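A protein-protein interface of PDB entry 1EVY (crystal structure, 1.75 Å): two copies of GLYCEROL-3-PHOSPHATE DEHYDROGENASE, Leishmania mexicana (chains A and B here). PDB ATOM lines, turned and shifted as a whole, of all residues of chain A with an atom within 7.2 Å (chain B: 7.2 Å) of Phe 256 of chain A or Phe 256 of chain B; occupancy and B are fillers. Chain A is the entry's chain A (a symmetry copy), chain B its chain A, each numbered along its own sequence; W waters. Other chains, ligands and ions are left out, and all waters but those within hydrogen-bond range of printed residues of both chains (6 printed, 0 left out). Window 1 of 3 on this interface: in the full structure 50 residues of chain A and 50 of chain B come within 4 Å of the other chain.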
ATOM      1  N   ASP A 199      10.994  24.672   1.089  1.00  0.00           N
ATOM      2  CA  ASP A 199      11.020  24.717  -0.372  1.00  0.00           C
ATOM      3  C   ASP A 199      10.426  25.899  -1.107  1.00  0.00           C
ATOM      4  O   ASP A 199       9.442  25.740  -1.844  1.00  0.00           O
ATOM      5  CB  ASP A 199      10.482  23.363  -0.918  1.00  0.00           C
ATOM      6  CG  ASP A 199      10.667  23.068  -2.398  1.00  0.00           C
ATOM      7  OD1 ASP A 199       9.983  22.234  -2.918  1.00  0.00           O
ATOM      8  OD2 ASP A 199      11.566  23.764  -3.067  1.00  0.00           O
ATOM      9  N   MET A 235      -1.169  13.591 -11.906  1.00  0.00           N
ATOM     10  CA  MET A 235       0.000  12.755 -11.516  1.00  0.00           C
ATOM     11  C   MET A 235       1.186  12.935 -12.433  1.00  0.00           C
ATOM     12  O   MET A 235       2.304  12.995 -11.970  1.00  0.00           O
ATOM     13  CB  MET A 235      -0.335  11.230 -11.375  1.00  0.00           C
ATOM     14  CG  MET A 235       0.751  10.208 -10.892  1.00  0.00           C
ATOM     15  SD  MET A 235       2.124   9.607 -11.991  1.00  0.00           S
ATOM     16  CE  MET A 235       3.396  10.454 -10.997  1.00  0.00           C
ATOM     17  N   ARG A 236       0.937  12.983 -13.751  1.00  0.00           N
ATOM     18  CA  ARG A 236       2.084  13.098 -14.625  1.00  0.00           C
ATOM     19  C   ARG A 236       2.606  14.574 -14.638  1.00  0.00           C
ATOM     20  O   ARG A 236       3.824  14.893 -14.791  1.00  0.00           O
ATOM     21  CB  ARG A 236       1.742  12.639 -16.062  1.00  0.00           C
ATOM     22  CG  ARG A 236       1.310  11.152 -16.152  1.00  0.00           C
ATOM     23  CD  ARG A 236       2.296  10.143 -15.561  1.00  0.00           C
ATOM     24  NE  ARG A 236       3.574  10.359 -16.219  1.00  0.00           N
ATOM     25  CZ  ARG A 236       4.662   9.754 -15.812  1.00  0.00           C
ATOM     26  NH1 ARG A 236       4.652   8.896 -14.852  1.00  0.00           N
ATOM     27  NH2 ARG A 236       5.814   9.995 -16.375  1.00  0.00           N
ATOM     28  N   LEU A 238       2.549  16.728 -12.221  1.00  0.00           N
ATOM     29  CA  LEU A 238       3.381  16.949 -11.062  1.00  0.00           C
ATOM     30  C   LEU A 238       4.843  16.638 -11.285  1.00  0.00           C
ATOM     31  O   LEU A 238       5.740  17.291 -10.709  1.00  0.00           O
ATOM     32  CB  LEU A 238       2.842  16.105  -9.921  1.00  0.00           C
ATOM     33  CG  LEU A 238       3.441  16.469  -8.575  1.00  0.00           C
ATOM     34  CD1 LEU A 238       2.980  17.869  -8.180  1.00  0.00           C
ATOM     35  CD2 LEU A 238       2.892  15.504  -7.559  1.00  0.00           C
ATOM     36  N   LEU A 239       5.137  15.601 -12.097  1.00  0.00           N
ATOM     37  CA  LEU A 239       6.550  15.322 -12.275  1.00  0.00           C
ATOM     38  C   LEU A 239       7.200  16.442 -13.051  1.00  0.00           C
ATOM     39  O   LEU A 239       8.402  16.607 -12.955  1.00  0.00           O
ATOM     40  CB  LEU A 239       6.797  13.967 -13.010  1.00  0.00           C
ATOM     41  CG  LEU A 239       6.084  12.786 -12.306  1.00  0.00           C
ATOM     42  CD1 LEU A 239       6.441  11.456 -12.978  1.00  0.00           C
ATOM     43  CD2 LEU A 239       6.440  12.755 -10.831  1.00  0.00           C
ATOM     44  N   ARG A 242       8.031  18.829 -10.573  1.00  0.00           N
ATOM     45  CA  ARG A 242       9.205  18.321  -9.876  1.00  0.00           C
ATOM     46  C   ARG A 242      10.477  18.562 -10.666  1.00  0.00           C
ATOM     47  O   ARG A 242      11.531  19.044 -10.180  1.00  0.00           O
ATOM     48  CB  ARG A 242       9.074  16.806  -9.679  1.00  0.00           C
ATOM     49  CG  ARG A 242      10.338  16.242  -9.093  1.00  0.00           C
ATOM     50  CD  ARG A 242      10.296  14.715  -9.103  1.00  0.00           C
ATOM     51  NE  ARG A 242      10.428  14.212 -10.488  1.00  0.00           N
ATOM     52  CZ  ARG A 242      10.349  12.914 -10.779  1.00  0.00           C
ATOM     53  NH1 ARG A 242      10.147  12.006  -9.860  1.00  0.00           N
ATOM     54  NH2 ARG A 242      10.469  12.523 -12.003  1.00  0.00           N
ATOM     55  N   GLY A 252      12.876  20.704  -3.582  1.00  0.00           N
ATOM     56  CA  GLY A 252      11.713  19.864  -3.955  1.00  0.00           C
ATOM     57  C   GLY A 252      10.841  19.330  -2.819  1.00  0.00           C
ATOM     58  O   GLY A 252       9.830  18.682  -3.109  1.00  0.00           O
ATOM     59  N   SER A 253      11.186  19.562  -1.537  1.00  0.00           N
ATOM     60  CA  SER A 253      10.333  19.077  -0.499  1.00  0.00           C
ATOM     61  C   SER A 253       8.896  19.605  -0.559  1.00  0.00           C
ATOM     62  O   SER A 253       8.029  19.080   0.109  1.00  0.00           O
ATOM     63  CB  SER A 253      10.967  19.179   0.883  1.00  0.00           C
ATOM     64  OG  SER A 253      11.098  20.532   1.109  1.00  0.00           O
ATOM     65  N   ALA A 254       8.535  20.584  -1.380  1.00  0.00           N
ATOM     66  CA  ALA A 254       7.109  20.975  -1.355  1.00  0.00           C
ATOM     67  C   ALA A 254       6.302  20.317  -2.456  1.00  0.00           C
ATOM     68  O   ALA A 254       5.066  20.385  -2.502  1.00  0.00           O
ATOM     69  CB  ALA A 254       6.919  22.494  -1.538  1.00  0.00           C
ATOM     70  N   VAL A 255       7.013  19.711  -3.394  1.00  0.00           N
ATOM     71  CA  VAL A 255       6.315  19.117  -4.571  1.00  0.00           C
ATOM     72  C   VAL A 255       5.161  18.210  -4.200  1.00  0.00           C
ATOM     73  O   VAL A 255       4.077  18.255  -4.779  1.00  0.00           O
ATOM     74  CB  VAL A 255       7.323  18.334  -5.454  1.00  0.00           C
ATOM     75  CG1 VAL A 255       6.696  17.730  -6.698  1.00  0.00           C
ATOM     76  CG2 VAL A 255       8.420  19.298  -5.846  1.00  0.00           C
ATOM     77  N   PHE A 256       5.465  17.329  -3.256  1.00  0.00           N
ATOM     78  CA  PHE A 256       4.453  16.374  -2.876  1.00  0.00           C
ATOM     79  C   PHE A 256       3.704  16.853  -1.662  1.00  0.00           C
ATOM     80  O   PHE A 256       3.040  16.063  -0.981  1.00  0.00           O
ATOM     81  CB  PHE A 256       5.032  14.943  -2.652  1.00  0.00           C
ATOM     82  CG  PHE A 256       5.663  14.439  -3.943  1.00  0.00           C
ATOM     83  CD1 PHE A 256       7.025  14.205  -4.025  1.00  0.00           C
ATOM     84  CD2 PHE A 256       4.890  14.236  -5.085  1.00  0.00           C
ATOM     85  CE1 PHE A 256       7.634  13.736  -5.187  1.00  0.00           C
ATOM     86  CE2 PHE A 256       5.482  13.795  -6.261  1.00  0.00           C
ATOM     87  CZ  PHE A 256       6.856  13.552  -6.321  1.00  0.00           C
ATOM     88  N   GLY A 257       3.792  18.151  -1.377  1.00  0.00           N
ATOM     89  CA  GLY A 257       3.043  18.618  -0.198  1.00  0.00           C
ATOM     90  C   GLY A 257       1.840  19.495  -0.607  1.00  0.00           C
ATOM     91  O   GLY A 257       1.337  19.459  -1.759  1.00  0.00           O
ATOM     92  N   LEU A 258       1.343  20.310   0.320  1.00  0.00           N
ATOM     93  CA  LEU A 258       0.168  21.118   0.001  1.00  0.00           C
ATOM     94  C   LEU A 258       0.318  22.104  -1.139  1.00  0.00           C
ATOM     95  O   LEU A 258      -0.594  22.326  -1.917  1.00  0.00           O
ATOM     96  CB  LEU A 258      -0.192  21.886   1.287  1.00  0.00           C
ATOM     97  CG  LEU A 258      -0.690  21.029   2.403  1.00  0.00           C
ATOM     98  CD1 LEU A 258      -0.516  21.774   3.755  1.00  0.00           C
ATOM     99  CD2 LEU A 258      -2.167  20.733   2.052  1.00  0.00           C
ATOM    100  N   ALA A 259       1.523  22.703  -1.250  1.00  0.00           N
ATOM    101  CA  ALA A 259       1.737  23.663  -2.274  1.00  0.00           C
ATOM    102  C   ALA A 259       1.885  23.050  -3.630  1.00  0.00           C
ATOM    103  O   ALA A 259       1.672  23.699  -4.605  1.00  0.00           O
ATOM    104  CB  ALA A 259       3.085  24.298  -1.937  1.00  0.00           C
ATOM    105  N   GLY A 260       2.338  21.775  -3.735  1.00  0.00           N
ATOM    106  CA  GLY A 260       2.526  21.190  -5.056  1.00  0.00           C
ATOM    107  C   GLY A 260       1.334  20.330  -5.319  1.00  0.00           C
ATOM    108  O   GLY A 260       0.358  20.768  -5.841  1.00  0.00           O
ATOM    109  N   LEU A 261       1.397  19.096  -4.869  1.00  0.00           N
ATOM    110  CA  LEU A 261       0.280  18.226  -5.130  1.00  0.00           C
ATOM    111  C   LEU A 261      -1.082  18.763  -4.709  1.00  0.00           C
ATOM    112  O   LEU A 261      -2.060  18.758  -5.476  1.00  0.00           O
ATOM    113  CB  LEU A 261       0.478  16.782  -4.516  1.00  0.00           C
ATOM    114  N   GLY A 262      -1.153  19.151  -3.446  1.00  0.00           N
ATOM    115  CA  GLY A 262      -2.418  19.616  -2.921  1.00  0.00           C
ATOM    116  C   GLY A 262      -3.032  20.699  -3.792  1.00  0.00           C
ATOM    117  O   GLY A 262      -4.187  20.618  -4.268  1.00  0.00           O
ATOM    118  N   GLU A 350       7.109   4.227 -14.561  1.00  0.00           N
ATOM    119  CA  GLU A 350       6.565   5.404 -13.935  1.00  0.00           C
ATOM    120  C   GLU A 350       7.523   6.570 -13.714  1.00  0.00           C
ATOM    121  O   GLU A 350       7.127   7.719 -13.810  1.00  0.00           O
ATOM    122  CB  GLU A 350       5.874   5.004 -12.654  1.00  0.00           C
ATOM    123  CG  GLU A 350       4.772   5.987 -12.320  1.00  0.00           C
ATOM    124  CD  GLU A 350       3.766   5.459 -11.328  1.00  0.00           C
ATOM    125  OE1 GLU A 350       3.966   4.655 -10.396  1.00  0.00           O
ATOM    126  OE2 GLU A 350       2.653   6.088 -11.517  1.00  0.00           O
ATOM    127  N   LEU A 352       9.362   7.306 -10.903  1.00  0.00           N
ATOM    128  CA  LEU A 352       9.428   7.696  -9.523  1.00  0.00           C
ATOM    129  C   LEU A 352      10.461   6.824  -8.777  1.00  0.00           C
ATOM    130  O   LEU A 352      10.410   5.587  -8.819  1.00  0.00           O
ATOM    131  CB  LEU A 352       8.059   7.552  -8.845  1.00  0.00           C
ATOM    132  CG  LEU A 352       7.098   8.657  -9.231  1.00  0.00           C
ATOM    133  CD1 LEU A 352       5.682   8.200  -8.946  1.00  0.00           C
ATOM    134  CD2 LEU A 352       7.349   9.892  -8.358  1.00  0.00           C
ATOM    135  N   PRO A 353      11.404   7.481  -8.057  1.00  0.00           N
ATOM    136  CA  PRO A 353      12.435   6.766  -7.299  1.00  0.00           C
ATOM    137  C   PRO A 353      11.908   6.107  -6.065  1.00  0.00           C
ATOM    138  O   PRO A 353      10.881   6.485  -5.495  1.00  0.00           O
ATOM    139  CB  PRO A 353      13.423   7.858  -6.854  1.00  0.00           C
ATOM    140  CG  PRO A 353      12.715   9.195  -7.038  1.00  0.00           C
ATOM    141  CD  PRO A 353      11.601   8.963  -8.053  1.00  0.00           C
ATOM    142  N   LEU A 355      11.431   5.504  -2.146  1.00  0.00           N
ATOM    143  CA  LEU A 355      11.546   6.354  -0.996  1.00  0.00           C
ATOM    144  C   LEU A 355      12.439   5.695   0.048  1.00  0.00           C
ATOM    145  O   LEU A 355      13.181   6.272   0.814  1.00  0.00           O
ATOM    146  CB  LEU A 355      10.160   6.516  -0.331  1.00  0.00           C
ATOM    147  CG  LEU A 355       9.208   7.276  -1.256  1.00  0.00           C
ATOM    148  CD1 LEU A 355       7.823   7.478  -0.677  1.00  0.00           C
ATOM    149  CD2 LEU A 355       9.873   8.572  -1.701  1.00  0.00           C
ATOM    150  N   ASP B 199       7.002  -1.108  -7.049  1.00  0.00           N
ATOM    151  CA  ASP B 199       6.407  -1.025  -5.716  1.00  0.00           C
ATOM    152  C   ASP B 199       5.138  -1.786  -5.401  1.00  0.00           C
ATOM    153  O   ASP B 199       4.100  -1.170  -5.119  1.00  0.00           O
ATOM    154  CB  ASP B 199       6.300   0.475  -5.315  1.00  0.00           C
ATOM    155  CG  ASP B 199       5.967   0.803  -3.869  1.00  0.00           C
ATOM    156  OD1 ASP B 199       5.540   1.889  -3.600  1.00  0.00           O
ATOM    157  OD2 ASP B 199       6.142  -0.136  -2.958  1.00  0.00           O
ATOM    158  N   MET B 235      -3.682  15.134   0.802  1.00  0.00           N
ATOM    159  CA  MET B 235      -2.226  15.377   1.003  1.00  0.00           C
ATOM    160  C   MET B 235      -1.708  14.812   2.304  1.00  0.00           C
ATOM    161  O   MET B 235      -0.632  14.257   2.335  1.00  0.00           O
ATOM    162  CB  MET B 235      -1.816  16.886   0.879  1.00  0.00           C
ATOM    163  CG  MET B 235      -0.314  17.322   0.979  1.00  0.00           C
ATOM    164  SD  MET B 235       0.603  17.406   2.593  1.00  0.00           S
ATOM    165  CE  MET B 235       1.699  16.024   2.132  1.00  0.00           C
ATOM    166  N   ARG B 236      -2.469  14.993   3.395  1.00  0.00           N
ATOM    167  CA  ARG B 236      -1.938  14.498   4.646  1.00  0.00           C
ATOM    168  C   ARG B 236      -2.124  12.946   4.735  1.00  0.00           C
ATOM    169  O   ARG B 236      -1.324  12.171   5.342  1.00  0.00           O
ATOM    170  CB  ARG B 236      -2.616  15.187   5.854  1.00  0.00           C
ATOM    171  CG  ARG B 236      -2.395  16.723   5.896  1.00  0.00           C
ATOM    172  CD  ARG B 236      -0.936  17.179   5.855  1.00  0.00           C
ATOM    173  NE  ARG B 236      -0.252  16.520   6.955  1.00  0.00           N
ATOM    174  CZ  ARG B 236       1.050  16.585   7.087  1.00  0.00           C
ATOM    175  NH1 ARG B 236       1.786  17.279   6.290  1.00  0.00           N
ATOM    176  NH2 ARG B 236       1.661  15.946   8.046  1.00  0.00           N
ATOM    177  N   LEU B 238      -2.065  10.792   2.318  1.00  0.00           N
ATOM    178  CA  LEU B 238      -1.004  10.143   1.586  1.00  0.00           C
ATOM    179  C   LEU B 238       0.225   9.846   2.414  1.00  0.00           C
ATOM    180  O   LEU B 238       0.923   8.833   2.198  1.00  0.00           O
ATOM    181  CB  LEU B 238      -0.631  11.025   0.407  1.00  0.00           C
ATOM    182  CG  LEU B 238       0.258  10.324  -0.604  1.00  0.00           C
ATOM    183  CD1 LEU B 238      -0.531   9.207  -1.281  1.00  0.00           C
ATOM    184  CD2 LEU B 238       0.622  11.332  -1.662  1.00  0.00           C
ATOM    185  N   LEU B 239       0.558  10.741   3.367  1.00  0.00           N
ATOM    186  CA  LEU B 239       1.752  10.432   4.133  1.00  0.00           C
ATOM    187  C   LEU B 239       1.505   9.220   4.999  1.00  0.00           C
ATOM    188  O   LEU B 239       2.457   8.569   5.388  1.00  0.00           O
ATOM    189  CB  LEU B 239       2.208  11.628   5.025  1.00  0.00           C
ATOM    190  CG  LEU B 239       2.399  12.927   4.204  1.00  0.00           C
ATOM    191  CD1 LEU B 239       2.961  14.050   5.083  1.00  0.00           C
ATOM    192  CD2 LEU B 239       3.305  12.673   3.013  1.00  0.00           C
ATOM    193  N   ARG B 242       2.216   6.485   2.869  1.00  0.00           N
ATOM    194  CA  ARG B 242       3.667   6.400   2.762  1.00  0.00           C
ATOM    195  C   ARG B 242       4.282   5.733   3.977  1.00  0.00           C
ATOM    196  O   ARG B 242       5.143   4.819   3.922  1.00  0.00           O
ATOM    197  CB  ARG B 242       4.262   7.811   2.669  1.00  0.00           C
ATOM    198  CG  ARG B 242       5.763   7.749   2.706  1.00  0.00           C
ATOM    199  CD  ARG B 242       6.351   9.154   2.839  1.00  0.00           C
ATOM    200  NE  ARG B 242       6.099   9.683   4.197  1.00  0.00           N
ATOM    201  CZ  ARG B 242       6.448  10.920   4.549  1.00  0.00           C
ATOM    202  NH1 ARG B 242       7.031  11.742   3.716  1.00  0.00           N
ATOM    203  NH2 ARG B 242       6.206  11.339   5.745  1.00  0.00           N
ATOM    204  N   GLY B 252       8.254   2.151  -1.673  1.00  0.00           N
ATOM    205  CA  GLY B 252       7.499   3.425  -1.732  1.00  0.00           C
ATOM    206  C   GLY B 252       7.470   4.162  -3.070  1.00  0.00           C
ATOM    207  O   GLY B 252       6.793   5.191  -3.160  1.00  0.00           O
ATOM    208  N   SER B 253       8.181   3.692  -4.115  1.00  0.00           N
ATOM    209  CA  SER B 253       8.108   4.386  -5.361  1.00  0.00           C
ATOM    210  C   SER B 253       6.696   4.502  -5.943  1.00  0.00           C
ATOM    211  O   SER B 253       6.477   5.272  -6.855  1.00  0.00           O
ATOM    212  CB  SER B 253       9.148   3.906  -6.366  1.00  0.00           C
ATOM    213  OG  SER B 253       8.792   2.603  -6.642  1.00  0.00           O
ATOM    214  N   ALA B 254       5.664   3.838  -5.435  1.00  0.00           N
ATOM    215  CA  ALA B 254       4.351   4.065  -6.077  1.00  0.00           C
ATOM    216  C   ALA B 254       3.513   5.095  -5.346  1.00  0.00           C
ATOM    217  O   ALA B 254       2.459   5.545  -5.816  1.00  0.00           O
ATOM    218  CB  ALA B 254       3.499   2.781  -6.129  1.00  0.00           C
ATOM    219  N   VAL B 255       3.958   5.440  -4.148  1.00  0.00           N
ATOM    220  CA  VAL B 255       3.152   6.373  -3.309  1.00  0.00           C
ATOM    221  C   VAL B 255       2.734   7.635  -4.034  1.00  0.00           C
ATOM    222  O   VAL B 255       1.596   8.092  -3.956  1.00  0.00           O
ATOM    223  CB  VAL B 255       3.935   6.752  -2.023  1.00  0.00           C
ATOM    224  CG1 VAL B 255       3.162   7.673  -1.095  1.00  0.00           C
ATOM    225  CG2 VAL B 255       4.273   5.464  -1.308  1.00  0.00           C
ATOM    226  N   PHE B 256       3.730   8.223  -4.685  1.00  0.00           N
ATOM    227  CA  PHE B 256       3.452   9.470  -5.356  1.00  0.00           C
ATOM    228  C   PHE B 256       3.141   9.230  -6.809  1.00  0.00           C
ATOM    229  O   PHE B 256       3.202  10.156  -7.626  1.00  0.00           O
ATOM    230  CB  PHE B 256       4.601  10.510  -5.191  1.00  0.00           C
ATOM    231  CG  PHE B 256       4.796  10.827  -3.714  1.00  0.00           C
ATOM    232  CD1 PHE B 256       5.968  10.489  -3.061  1.00  0.00           C
ATOM    233  CD2 PHE B 256       3.782  11.434  -2.975  1.00  0.00           C
ATOM    234  CE1 PHE B 256       6.183  10.772  -1.714  1.00  0.00           C
ATOM    235  CE2 PHE B 256       3.965  11.701  -1.624  1.00  0.00           C
ATOM    236  CZ  PHE B 256       5.160  11.363  -0.985  1.00  0.00           C
ATOM    237  N   GLY B 257       2.796   7.990  -7.151  1.00  0.00           N
ATOM    238  CA  GLY B 257       2.476   7.764  -8.571  1.00  0.00           C
ATOM    239  C   GLY B 257       0.969   7.500  -8.773  1.00  0.00           C
ATOM    240  O   GLY B 257       0.102   7.846  -7.929  1.00  0.00           O
ATOM    241  N   LEU B 258       0.608   6.879  -9.893  1.00  0.00           N
ATOM    242  CA  LEU B 258      -0.812   6.657 -10.158  1.00  0.00           C
ATOM    243  C   LEU B 258      -1.560   5.806  -9.152  1.00  0.00           C
ATOM    244  O   LEU B 258      -2.713   6.051  -8.839  1.00  0.00           O
ATOM    245  CB  LEU B 258      -0.895   5.989 -11.543  1.00  0.00           C
ATOM    246  CG  LEU B 258      -0.494   6.867 -12.681  1.00  0.00           C
ATOM    247  CD1 LEU B 258      -0.105   5.996 -13.906  1.00  0.00           C
ATOM    248  CD2 LEU B 258      -1.719   7.775 -12.938  1.00  0.00           C
ATOM    249  N   ALA B 259      -0.869   4.779  -8.614  1.00  0.00           N
ATOM    250  CA  ALA B 259      -1.507   3.914  -7.686  1.00  0.00           C
ATOM    251  C   ALA B 259      -1.689   4.536  -6.337  1.00  0.00           C
ATOM    252  O   ALA B 259      -2.527   4.124  -5.599  1.00  0.00           O
ATOM    253  CB  ALA B 259      -0.530   2.754  -7.499  1.00  0.00           C
ATOM    254  N   GLY B 260      -0.839   5.515  -5.939  1.00  0.00           N
ATOM    255  CA  GLY B 260      -0.985   6.092  -4.609  1.00  0.00           C
ATOM    256  C   GLY B 260      -1.713   7.385  -4.778  1.00  0.00           C
ATOM    257  O   GLY B 260      -2.901   7.436  -4.744  1.00  0.00           O
ATOM    258  N   LEU B 261      -0.971   8.438  -5.047  1.00  0.00           N
ATOM    259  CA  LEU B 261      -1.632   9.709  -5.186  1.00  0.00           C
ATOM    260  C   LEU B 261      -2.791   9.741  -6.175  1.00  0.00           C
ATOM    261  O   LEU B 261      -3.899  10.218  -5.877  1.00  0.00           O
ATOM    262  CB  LEU B 261      -0.627  10.881  -5.529  1.00  0.00           C
ATOM    263  N   GLY B 262      -2.491   9.302  -7.386  1.00  0.00           N
ATOM    264  CA  GLY B 262      -3.499   9.350  -8.423  1.00  0.00           C
ATOM    265  C   GLY B 262      -4.799   8.700  -7.982  1.00  0.00           C
ATOM    266  O   GLY B 262      -5.902   9.291  -8.015  1.00  0.00           O
ATOM    267  N   GLU B 350       5.824  20.481   7.461  1.00  0.00           N
ATOM    268  CA  GLU B 350       5.153  19.578   6.562  1.00  0.00           C
ATOM    269  C   GLU B 350       5.546  18.107   6.644  1.00  0.00           C
ATOM    270  O   GLU B 350       4.713  17.236   6.464  1.00  0.00           O
ATOM    271  CB  GLU B 350       5.277  20.107   5.152  1.00  0.00           C
ATOM    272  CG  GLU B 350       4.112  19.635   4.309  1.00  0.00           C
ATOM    273  CD  GLU B 350       3.914  20.435   3.045  1.00  0.00           C
ATOM    274  OE1 GLU B 350       4.787  20.997   2.355  1.00  0.00           O
ATOM    275  OE2 GLU B 350       2.671  20.339   2.704  1.00  0.00           O
ATOM    276  N   LEU B 352       7.893  16.425   4.776  1.00  0.00           N
ATOM    277  CA  LEU B 352       8.350  15.917   3.514  1.00  0.00           C
ATOM    278  C   LEU B 352       9.855  16.216   3.339  1.00  0.00           C
ATOM    279  O   LEU B 352      10.304  17.363   3.470  1.00  0.00           O
ATOM    280  CB  LEU B 352       7.570  16.546   2.352  1.00  0.00           C
ATOM    281  CG  LEU B 352       6.176  15.974   2.208  1.00  0.00           C
ATOM    282  CD1 LEU B 352       5.325  16.942   1.412  1.00  0.00           C
ATOM    283  CD2 LEU B 352       6.231  14.670   1.404  1.00  0.00           C
ATOM    284  N   PRO B 353      10.649  15.166   3.010  1.00  0.00           N
ATOM    285  CA  PRO B 353      12.093  15.322   2.809  1.00  0.00           C
ATOM    286  C   PRO B 353      12.438  16.022   1.535  1.00  0.00           C
ATOM    287  O   PRO B 353      11.678  16.048   0.562  1.00  0.00           O
ATOM    288  CB  PRO B 353      12.632  13.885   2.708  1.00  0.00           C
ATOM    289  CG  PRO B 353      11.431  12.979   2.462  1.00  0.00           C
ATOM    290  CD  PRO B 353      10.204  13.740   2.950  1.00  0.00           C
ATOM    291  N   LEU B 355      13.897  16.403  -2.164  1.00  0.00           N
ATOM    292  CA  LEU B 355      14.113  15.479  -3.240  1.00  0.00           C
ATOM    293  C   LEU B 355      15.537  15.614  -3.761  1.00  0.00           C
ATOM    294  O   LEU B 355      16.219  14.716  -4.207  1.00  0.00           O
ATOM    295  CB  LEU B 355      13.188  15.838  -4.425  1.00  0.00           C
ATOM    296  CG  LEU B 355      11.722  15.625  -4.044  1.00  0.00           C
ATOM    297  CD1 LEU B 355      10.746  15.956  -5.155  1.00  0.00           C
ATOM    298  CD2 LEU B 355      11.551  14.217  -3.488  1.00  0.00           C
HETATM  299  O   HOH W   1       3.322  12.779  -8.854  1.00  0.00           O
HETATM  300  O   HOH W   2       3.931  22.285  -0.050  1.00  0.00           O
HETATM  301  O   HOH W   3       1.560  13.747  -0.059  1.00  0.00           O
HETATM  302  O   HOH W   4       6.175   3.976  -9.296  1.00  0.00           O
HETATM  303  O   HOH W   5       1.757   4.059  -8.681  1.00  0.00           O
HETATM  304  O   HOH W   6       7.317  20.605   2.322  1.00  0.00           O
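N of Leu 258 of chain A is in hydrogen-bond range of OE2 of Glu 350 of chain B (2.7 Å). N of Leu 258 of chain B lies within hydrogen-bond range of OE2 of Glu 350 of chain A (2.7 Å). The backbone NH (N) of Leu 258 of chain A lies close to the side-chain sulfur (SD) of Met 235 of chain B, 3.8 Å away. The backbone NH (N) of Leu 258 of chain B sits close to the side-chain sulfur (SD) of Met 235 of chain A.
The guanidinium group of Arg 236 of chain A lies within hydrogen-bond range of the backbone carbonyl oxygen of Glu 350 of chain A. OD1 of Asp 199 of chain B lies close to N of Gly 252 of chain B, 3.3 Å away. NH1 of Arg 236 of chain B sits at hydrogen-bond distance from O of Glu 350 of chain B, 2.9 Å away.
Ser 253 of chain A touches Leu 352 of chain B, and with the chains exchanged Leu 352 of chain A touches Ser 253 of chain B. Gly 257 of chain A touches Glu 350 of chain B, and with the chains exchanged Glu 350 of chain A touches Gly 257 of chain B.
Of the printed residues of chain B, Phe 256 of chain A touches Met 235 (3.4 Å), Phe 256 (3.6 Å), Leu 352 (3.4 Å) and Leu 355 (3.8 Å). Of the printed residues of chain A, Arg 242 of chain B touches Leu 355. Printed residues of chain A within 4 Å of Pro 353 of chain B: Ser 253. The nearest printed residue of chain B that does not touch Phe 256 of chain A is Leu 239 of chain B (5.2 Å). The nearest printed residue of chain A that does not touch Phe 256 of chain B is Leu 239 of chain A (5.2 Å). The nearest printed residue of chain B that does not touch Ser 253 of chain A is Leu 355 of chain B (4.2 Å).
Water W3 lies within hydrogen-bond range of the backbone carbonyl oxygen (O) of Phe 256 of chain A (2.9 Å) and the backbone carbonyl oxygen (O) of Met 235 of chain B (3.3 Å).
Among the printed residues, merely in contact across the chains: Met 235 of chain A with Phe 256 of chain B, Met 235 of chain A with Gly 257 of chain B, Arg 242 of chain A with Leu 355 of chain B, Gly 252 of chain A with Leu 355 of chain B, Ser 253 of chain A with Leu 352 of chain B, Ser 253 of chain A with Pro 353 of chain B, Phe 256 of chain A with Met 235 of chain B, Phe 256 of chain A with Phe 256 of chain B, Phe 256 of chain A with Leu 352 of chain B, Phe 256 of chain A with Leu 355 of chain B, Gly 257 of chain A with Met 235 of chain B, Gly 257 of chain A with Glu 350 of chain B, Gly 257 of chain A with Leu 352 of chain B, Glu 350 of chain A with Gly 257 of chain B, Leu 352 of chain A with Ser 253 of chain B, Leu 352 of chain A with Phe 256 of chain B, Leu 352 of chain A with Gly 257 of chain B, Pro 353 of chain A with Ser 253 of chain B, Leu 355 of chain A with Arg 242 of chain B, Leu 355 of chain A with Gly 252 of chain B and Leu 355 of chain A with Phe 256 of chain B.
Of the 21 printed residues of chain B, 11 touch a printed residue of chain A. Hydrophobic or aromatic side chains of chain B within 4 Å of the printed part of chain A: Met 235, Phe 256, Leu 258, Leu 352 and Leu 355. Along chain B the printed residues that touch a printed residue of chain A span positions 235 to 355. Printed residues of chain A that touch a printed residue of chain B: Met 235, Arg 242, Gly 252, Ser 253, Phe 256, Gly 257, Leu 258, Glu 350, Leu 352, Pro 353 and Leu 355. Hydrophobic or aromatic side chains of chain A within 4 Å of the printed part of chain B: Met 235, Phe 256, Leu 258, Leu 352 and Leu 355.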
